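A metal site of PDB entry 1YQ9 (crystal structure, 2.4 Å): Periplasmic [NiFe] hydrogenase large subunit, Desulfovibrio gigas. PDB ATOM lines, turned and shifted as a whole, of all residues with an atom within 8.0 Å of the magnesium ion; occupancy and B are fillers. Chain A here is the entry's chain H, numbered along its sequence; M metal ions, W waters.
Water W1 lies within hydrogen-bond range of the side-chain amide nitrogen of Gln 481 (2.6 Å), the side-chain carboxylate of Glu 321 (2.6 Å) and the side-chain amino group of Lys 358 (3.1 Å). Water W3 bridges OE2 of Glu 46 and NZ of Lys 358.
OE1 of Glu 46 lies close to NE2 of Gln 481 (3.3 Å). A ring nitrogen (ND1) of His 536 lies within hydrogen-bond range of the backbone carbonyl oxygen (O) of Cys 533 (2.8 Å). The side-chain carboxylate (OE2) of Glu 46 is in hydrogen-bond range of the side-chain hydroxyl (OG1) of Thr 341, at 2.7 Å.
The magnesium ion is bound by O of Leu 482 (2.1 Å). The magnesium ion is bound by water W1 (2.1 Å). Water W2 binds the magnesium ion. NE2 of His 536 is bound to the magnesium ion, 2.1 Å away. OE1 of Glu 46 is bound to the magnesium ion (2.1 Å). Water W3 is bound to the magnesium ion, at 2.1 Å.
Within 4 Å of the magnesium ion: Glu 46, Leu 482 and His 536.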
ATOM      1  N   GLU A  46      18.672   9.567 -11.335  1.00  0.00           N
ATOM      2  CA  GLU A  46      18.794   9.920 -12.751  1.00  0.00           C
ATOM      3  C   GLU A  46      18.945  11.426 -12.948  1.00  0.00           C
ATOM      4  O   GLU A  46      19.718  11.857 -13.807  1.00  0.00           O
ATOM      5  CB  GLU A  46      17.599   9.382 -13.566  1.00  0.00           C
ATOM      6  CG  GLU A  46      17.478   7.864 -13.569  1.00  0.00           C
ATOM      7  CD  GLU A  46      16.037   7.356 -13.619  1.00  0.00           C
ATOM      8  OE1 GLU A  46      15.854   6.182 -13.975  1.00  0.00           O
ATOM      9  OE2 GLU A  46      15.083   8.117 -13.299  1.00  0.00           O
ATOM     10  N   GLU A 321       8.430   2.772 -20.340  1.00  0.00           N
ATOM     11  CA  GLU A 321       8.032   3.072 -18.972  1.00  0.00           C
ATOM     12  C   GLU A 321       6.919   4.100 -18.941  1.00  0.00           C
ATOM     13  O   GLU A 321       7.060   5.184 -19.518  1.00  0.00           O
ATOM     14  CB  GLU A 321       9.216   3.591 -18.161  1.00  0.00           C
ATOM     15  CG  GLU A 321      10.335   2.580 -17.996  1.00  0.00           C
ATOM     16  CD  GLU A 321      11.367   3.056 -17.000  1.00  0.00           C
ATOM     17  OE1 GLU A 321      12.152   3.962 -17.336  1.00  0.00           O
ATOM     18  OE2 GLU A 321      11.405   2.510 -15.878  1.00  0.00           O
ATOM     19  N   TYR A 328       4.858  11.777 -11.787  1.00  0.00           N
ATOM     20  CA  TYR A 328       5.710  12.436 -12.765  1.00  0.00           C
ATOM     21  C   TYR A 328       4.842  13.269 -13.697  1.00  0.00           C
ATOM     22  O   TYR A 328       3.609  13.130 -13.721  1.00  0.00           O
ATOM     23  CB  TYR A 328       6.543  11.425 -13.553  1.00  0.00           C
ATOM     24  CG  TYR A 328       7.480  10.630 -12.669  1.00  0.00           C
ATOM     25  CD1 TYR A 328       8.729  11.126 -12.299  1.00  0.00           C
ATOM     26  CD2 TYR A 328       7.095   9.382 -12.175  1.00  0.00           C
ATOM     27  CE1 TYR A 328       9.573  10.389 -11.449  1.00  0.00           C
ATOM     28  CE2 TYR A 328       7.931   8.649 -11.347  1.00  0.00           C
ATOM     29  CZ  TYR A 328       9.167   9.156 -10.987  1.00  0.00           C
ATOM     30  OH  TYR A 328       9.992   8.404 -10.165  1.00  0.00           O
ATOM     31  N   PRO A 336      13.723   3.553 -22.589  1.00  0.00           N
ATOM     32  CA  PRO A 336      14.727   4.153 -21.699  1.00  0.00           C
ATOM     33  C   PRO A 336      15.810   5.025 -22.364  1.00  0.00           C
ATOM     34  O   PRO A 336      16.323   5.907 -21.693  1.00  0.00           O
ATOM     35  CB  PRO A 336      15.368   2.945 -21.001  1.00  0.00           C
ATOM     36  CG  PRO A 336      14.357   1.873 -21.125  1.00  0.00           C
ATOM     37  CD  PRO A 336      13.677   2.090 -22.444  1.00  0.00           C
ATOM     38  N   GLY A 339      14.234   8.039 -21.972  1.00  0.00           N
ATOM     39  CA  GLY A 339      13.562   8.172 -20.688  1.00  0.00           C
ATOM     40  C   GLY A 339      13.549   9.600 -20.194  1.00  0.00           C
ATOM     41  O   GLY A 339      14.492  10.351 -20.430  1.00  0.00           O
ATOM     42  N   VAL A 340      12.475   9.971 -19.508  1.00  0.00           N
ATOM     43  CA  VAL A 340      12.335  11.297 -18.900  1.00  0.00           C
ATOM     44  C   VAL A 340      12.027  11.165 -17.392  1.00  0.00           C
ATOM     45  O   VAL A 340      11.186  10.352 -17.008  1.00  0.00           O
ATOM     46  CB  VAL A 340      11.184  12.080 -19.548  1.00  0.00           C
ATOM     47  CG1 VAL A 340      11.019  13.435 -18.880  1.00  0.00           C
ATOM     48  CG2 VAL A 340      11.434  12.237 -21.033  1.00  0.00           C
ATOM     49  N   THR A 341      12.702  11.953 -16.565  1.00  0.00           N
ATOM     50  CA  THR A 341      12.455  11.901 -15.130  1.00  0.00           C
ATOM     51  C   THR A 341      12.131  13.270 -14.570  1.00  0.00           C
ATOM     52  O   THR A 341      13.022  14.025 -14.174  1.00  0.00           O
ATOM     53  CB  THR A 341      13.653  11.290 -14.428  1.00  0.00           C
ATOM     54  OG1 THR A 341      13.806   9.939 -14.909  1.00  0.00           O
ATOM     55  CG2 THR A 341      13.362  11.112 -12.950  1.00  0.00           C
ATOM     56  N   TRP A 356       5.768   6.597  -6.637  1.00  0.00           N
ATOM     57  CA  TRP A 356       7.005   7.177  -7.179  1.00  0.00           C
ATOM     58  C   TRP A 356       7.713   6.244  -8.167  1.00  0.00           C
ATOM     59  O   TRP A 356       8.711   6.646  -8.791  1.00  0.00           O
ATOM     60  CB  TRP A 356       7.986   7.531  -6.071  1.00  0.00           C
ATOM     61  CG  TRP A 356       7.593   8.743  -5.261  1.00  0.00           C
ATOM     62  CD1 TRP A 356       7.246   8.776  -3.935  1.00  0.00           C
ATOM     63  CD2 TRP A 356       7.525  10.100  -5.723  1.00  0.00           C
ATOM     64  NE1 TRP A 356       6.961  10.061  -3.562  1.00  0.00           N
ATOM     65  CE2 TRP A 356       7.131  10.901  -4.638  1.00  0.00           C
ATOM     66  CE3 TRP A 356       7.761  10.723  -6.961  1.00  0.00           C
ATOM     67  CZ2 TRP A 356       6.955  12.282  -4.737  1.00  0.00           C
ATOM     68  CZ3 TRP A 356       7.604  12.095  -7.055  1.00  0.00           C
ATOM     69  CH2 TRP A 356       7.205  12.857  -5.945  1.00  0.00           C
ATOM     70  N   MET A 357       7.241   5.010  -8.297  1.00  0.00           N
ATOM     71  CA  MET A 357       7.728   4.128  -9.370  1.00  0.00           C
ATOM     72  C   MET A 357       7.086   4.440 -10.718  1.00  0.00           C
ATOM     73  O   MET A 357       5.888   4.738 -10.788  1.00  0.00           O
ATOM     74  CB  MET A 357       7.465   2.660  -9.036  1.00  0.00           C
ATOM     75  CG  MET A 357       8.337   2.126  -7.928  1.00  0.00           C
ATOM     76  SD  MET A 357       8.357   0.342  -7.936  1.00  0.00           S
ATOM     77  CE  MET A 357       9.065   0.000  -6.343  1.00  0.00           C
ATOM     78  N   LYS A 358       7.862   4.373 -11.787  1.00  0.00           N
ATOM     79  CA  LYS A 358       7.315   4.329 -13.132  1.00  0.00           C
ATOM     80  C   LYS A 358       6.768   2.913 -13.365  1.00  0.00           C
ATOM     81  O   LYS A 358       6.988   2.003 -12.543  1.00  0.00           O
ATOM     82  CB  LYS A 358       8.409   4.629 -14.162  1.00  0.00           C
ATOM     83  CG  LYS A 358       9.096   5.972 -13.986  1.00  0.00           C
ATOM     84  CD  LYS A 358      10.036   6.280 -15.135  1.00  0.00           C
ATOM     85  CE  LYS A 358      10.824   7.568 -14.916  1.00  0.00           C
ATOM     86  NZ  LYS A 358      11.967   7.691 -15.880  1.00  0.00           N
ATOM     87  N   PRO A 360       6.976  -0.034 -15.957  1.00  0.00           N
ATOM     88  CA  PRO A 360       7.565  -0.695 -17.128  1.00  0.00           C
ATOM     89  C   PRO A 360       6.632  -1.704 -17.738  1.00  0.00           C
ATOM     90  O   PRO A 360       6.057  -2.531 -17.006  1.00  0.00           O
ATOM     91  CB  PRO A 360       8.798  -1.398 -16.542  1.00  0.00           C
ATOM     92  CG  PRO A 360       9.046  -0.664 -15.255  1.00  0.00           C
ATOM     93  CD  PRO A 360       7.674  -0.380 -14.711  1.00  0.00           C
ATOM     94  N   SER A 467      18.505  -3.089 -16.068  1.00  0.00           N
ATOM     95  CA  SER A 467      19.137  -2.475 -17.227  1.00  0.00           C
ATOM     96  C   SER A 467      19.416  -0.992 -16.989  1.00  0.00           C
ATOM     97  O   SER A 467      18.537  -0.244 -16.530  1.00  0.00           O
ATOM     98  CB  SER A 467      18.292  -2.664 -18.493  1.00  0.00           C
ATOM     99  OG  SER A 467      16.991  -2.102 -18.366  1.00  0.00           O
ATOM    100  N   TRP A 469      20.898   2.482 -18.978  1.00  0.00           N
ATOM    101  CA  TRP A 469      20.915   2.979 -20.348  1.00  0.00           C
ATOM    102  C   TRP A 469      21.572   4.342 -20.396  1.00  0.00           C
ATOM    103  O   TRP A 469      21.080   5.281 -19.766  1.00  0.00           O
ATOM    104  CB  TRP A 469      19.494   3.097 -20.879  1.00  0.00           C
ATOM    105  CG  TRP A 469      18.630   1.851 -20.739  1.00  0.00           C
ATOM    106  CD1 TRP A 469      18.073   1.358 -19.591  1.00  0.00           C
ATOM    107  CD2 TRP A 469      18.207   0.976 -21.796  1.00  0.00           C
ATOM    108  NE1 TRP A 469      17.347   0.225 -19.868  1.00  0.00           N
ATOM    109  CE2 TRP A 469      17.414  -0.037 -21.218  1.00  0.00           C
ATOM    110  CE3 TRP A 469      18.440   0.933 -23.174  1.00  0.00           C
ATOM    111  CZ2 TRP A 469      16.850  -1.071 -21.955  1.00  0.00           C
ATOM    112  CZ3 TRP A 469      17.880  -0.107 -23.923  1.00  0.00           C
ATOM    113  CH2 TRP A 469      17.081  -1.091 -23.310  1.00  0.00           C
ATOM    114  N   PHE A 480      20.806   9.159 -18.596  1.00  0.00           N
ATOM    115  CA  PHE A 480      21.142   7.923 -17.920  1.00  0.00           C
ATOM    116  C   PHE A 480      19.923   7.446 -17.169  1.00  0.00           C
ATOM    117  O   PHE A 480      19.488   8.106 -16.227  1.00  0.00           O
ATOM    118  CB  PHE A 480      22.303   8.128 -16.975  1.00  0.00           C
ATOM    119  CG  PHE A 480      22.997   6.855 -16.592  1.00  0.00           C
ATOM    120  CD1 PHE A 480      22.355   5.901 -15.827  1.00  0.00           C
ATOM    121  CD2 PHE A 480      24.291   6.604 -17.025  1.00  0.00           C
ATOM    122  CE1 PHE A 480      22.990   4.720 -15.506  1.00  0.00           C
ATOM    123  CE2 PHE A 480      24.935   5.426 -16.693  1.00  0.00           C
ATOM    124  CZ  PHE A 480      24.282   4.491 -15.934  1.00  0.00           C
ATOM    125  N   GLN A 481      19.372   6.305 -17.578  1.00  0.00           N
ATOM    126  CA  GLN A 481      18.126   5.803 -17.003  1.00  0.00           C
ATOM    127  C   GLN A 481      18.294   4.420 -16.411  1.00  0.00           C
ATOM    128  O   GLN A 481      18.951   3.567 -17.013  1.00  0.00           O
ATOM    129  CB  GLN A 481      17.024   5.759 -18.070  1.00  0.00           C
ATOM    130  CG  GLN A 481      16.651   7.110 -18.682  1.00  0.00           C
ATOM    131  CD  GLN A 481      15.806   7.953 -17.725  1.00  0.00           C
ATOM    132  OE1 GLN A 481      15.944   9.179 -17.674  1.00  0.00           O
ATOM    133  NE2 GLN A 481      14.942   7.297 -16.972  1.00  0.00           N
ATOM    134  N   LEU A 482      17.697   4.183 -15.244  1.00  0.00           N
ATOM    135  CA  LEU A 482      17.637   2.820 -14.741  1.00  0.00           C
ATOM    136  C   LEU A 482      16.210   2.272 -14.792  1.00  0.00           C
ATOM    137  O   LEU A 482      15.245   2.985 -14.486  1.00  0.00           O
ATOM    138  CB  LEU A 482      18.210   2.679 -13.329  1.00  0.00           C
ATOM    139  CG  LEU A 482      19.137   3.716 -12.684  1.00  0.00           C
ATOM    140  CD1 LEU A 482      19.755   3.112 -11.423  1.00  0.00           C
ATOM    141  CD2 LEU A 482      20.210   4.233 -13.626  1.00  0.00           C
ATOM    142  N   VAL A 483      16.092   1.001 -15.174  1.00  0.00           N
ATOM    143  CA  VAL A 483      14.835   0.286 -15.131  1.00  0.00           C
ATOM    144  C   VAL A 483      15.142  -0.982 -14.375  1.00  0.00           C
ATOM    145  O   VAL A 483      15.948  -1.808 -14.836  1.00  0.00           O
ATOM    146  CB  VAL A 483      14.303  -0.044 -16.549  1.00  0.00           C
ATOM    147  CG1 VAL A 483      12.873  -0.622 -16.476  1.00  0.00           C
ATOM    148  CG2 VAL A 483      14.354   1.196 -17.442  1.00  0.00           C
ATOM    149  N   VAL A 484      14.535  -1.126 -13.199  1.00  0.00           N
ATOM    150  CA  VAL A 484      15.035  -2.135 -12.262  1.00  0.00           C
ATOM    151  C   VAL A 484      13.948  -3.136 -11.848  1.00  0.00           C
ATOM    152  O   VAL A 484      12.749  -2.853 -11.970  1.00  0.00           O
ATOM    153  CB  VAL A 484      15.926  -1.483 -11.126  1.00  0.00           C
ATOM    154  CG1 VAL A 484      15.901   0.060 -11.197  1.00  0.00           C
ATOM    155  CG2 VAL A 484      15.619  -2.018  -9.750  1.00  0.00           C
ATOM    156  N   THR A 487      10.970  -2.249 -10.122  1.00  0.00           N
ATOM    157  CA  THR A 487      10.158  -1.307 -10.906  1.00  0.00           C
ATOM    158  C   THR A 487       9.110  -2.102 -11.686  1.00  0.00           C
ATOM    159  O   THR A 487       7.944  -1.733 -11.710  1.00  0.00           O
ATOM    160  CB  THR A 487      10.985  -0.448 -11.900  1.00  0.00           C
ATOM    161  OG1 THR A 487      12.102   0.168 -11.248  1.00  0.00           O
ATOM    162  CG2 THR A 487      10.136   0.750 -12.387  1.00  0.00           C
ATOM    163  N   CYS A 533      15.626   0.466  -4.959  1.00  0.00           N
ATOM    164  CA  CYS A 533      15.818  -0.030  -6.318  1.00  0.00           C
ATOM    165  C   CYS A 533      14.722   0.443  -7.280  1.00  0.00           C
ATOM    166  O   CYS A 533      15.011   1.032  -8.319  1.00  0.00           O
ATOM    167  CB  CYS A 533      15.866  -1.566  -6.342  1.00  0.00           C
ATOM    168  SG  CYS A 533      17.531  -2.251  -6.239  1.00  0.00           S
ATOM    169  N   GLY A 534      13.469   0.178  -6.916  1.00  0.00           N
ATOM    170  CA  GLY A 534      12.360   0.430  -7.835  1.00  0.00           C
ATOM    171  C   GLY A 534      12.197   1.874  -8.261  1.00  0.00           C
ATOM    172  O   GLY A 534      11.851   2.137  -9.427  1.00  0.00           O
ATOM    173  N   VAL A 535      12.444   2.794  -7.334  1.00  0.00           N
ATOM    174  CA  VAL A 535      12.255   4.215  -7.583  1.00  0.00           C
ATOM    175  C   VAL A 535      13.561   4.938  -7.997  1.00  0.00           C
ATOM    176  O   VAL A 535      13.561   5.788  -8.890  1.00  0.00           O
ATOM    177  CB  VAL A 535      11.634   4.940  -6.347  1.00  0.00           C
ATOM    178  CG1 VAL A 535      11.370   6.410  -6.661  1.00  0.00           C
ATOM    179  CG2 VAL A 535      10.355   4.256  -5.891  1.00  0.00           C
ATOM    180  N   HIS A 536      14.661   4.586  -7.353  1.00  0.00           N
ATOM    181  CA  HIS A 536      15.920   5.316  -7.495  1.00  0.00           C
ATOM    182  C   HIS A 536      15.723   6.846  -7.591  1.00  0.00           C
ATOM    183  O   HIS A 536      16.220   7.512  -8.512  1.00  0.00           O
ATOM    184  CB  HIS A 536      16.739   4.762  -8.680  1.00  0.00           C
ATOM    185  CG  HIS A 536      15.924   4.449  -9.898  1.00  0.00           C
ATOM    186  ND1 HIS A 536      15.185   3.290 -10.017  1.00  0.00           N
ATOM    187  CD2 HIS A 536      15.776   5.114 -11.067  1.00  0.00           C
ATOM    188  CE1 HIS A 536      14.590   3.267 -11.208  1.00  0.00           C
ATOM    189  NE2 HIS A 536      14.925   4.372 -11.856  1.00  0.00           N
ATOM    190  OXT HIS A 536      15.065   7.483  -6.749  1.00  0.00           O
HETATM  191 MG    MG M   1      14.325   4.735 -13.842  1.00  0.00          MG
HETATM  192  O   HOH W   1      13.863   5.271 -15.812  1.00  0.00           O
HETATM  193  O   HOH W   2      12.641   3.481 -13.700  1.00  0.00           O
HETATM  194  O   HOH W   3      13.217   6.474 -13.254  1.00  0.00           O
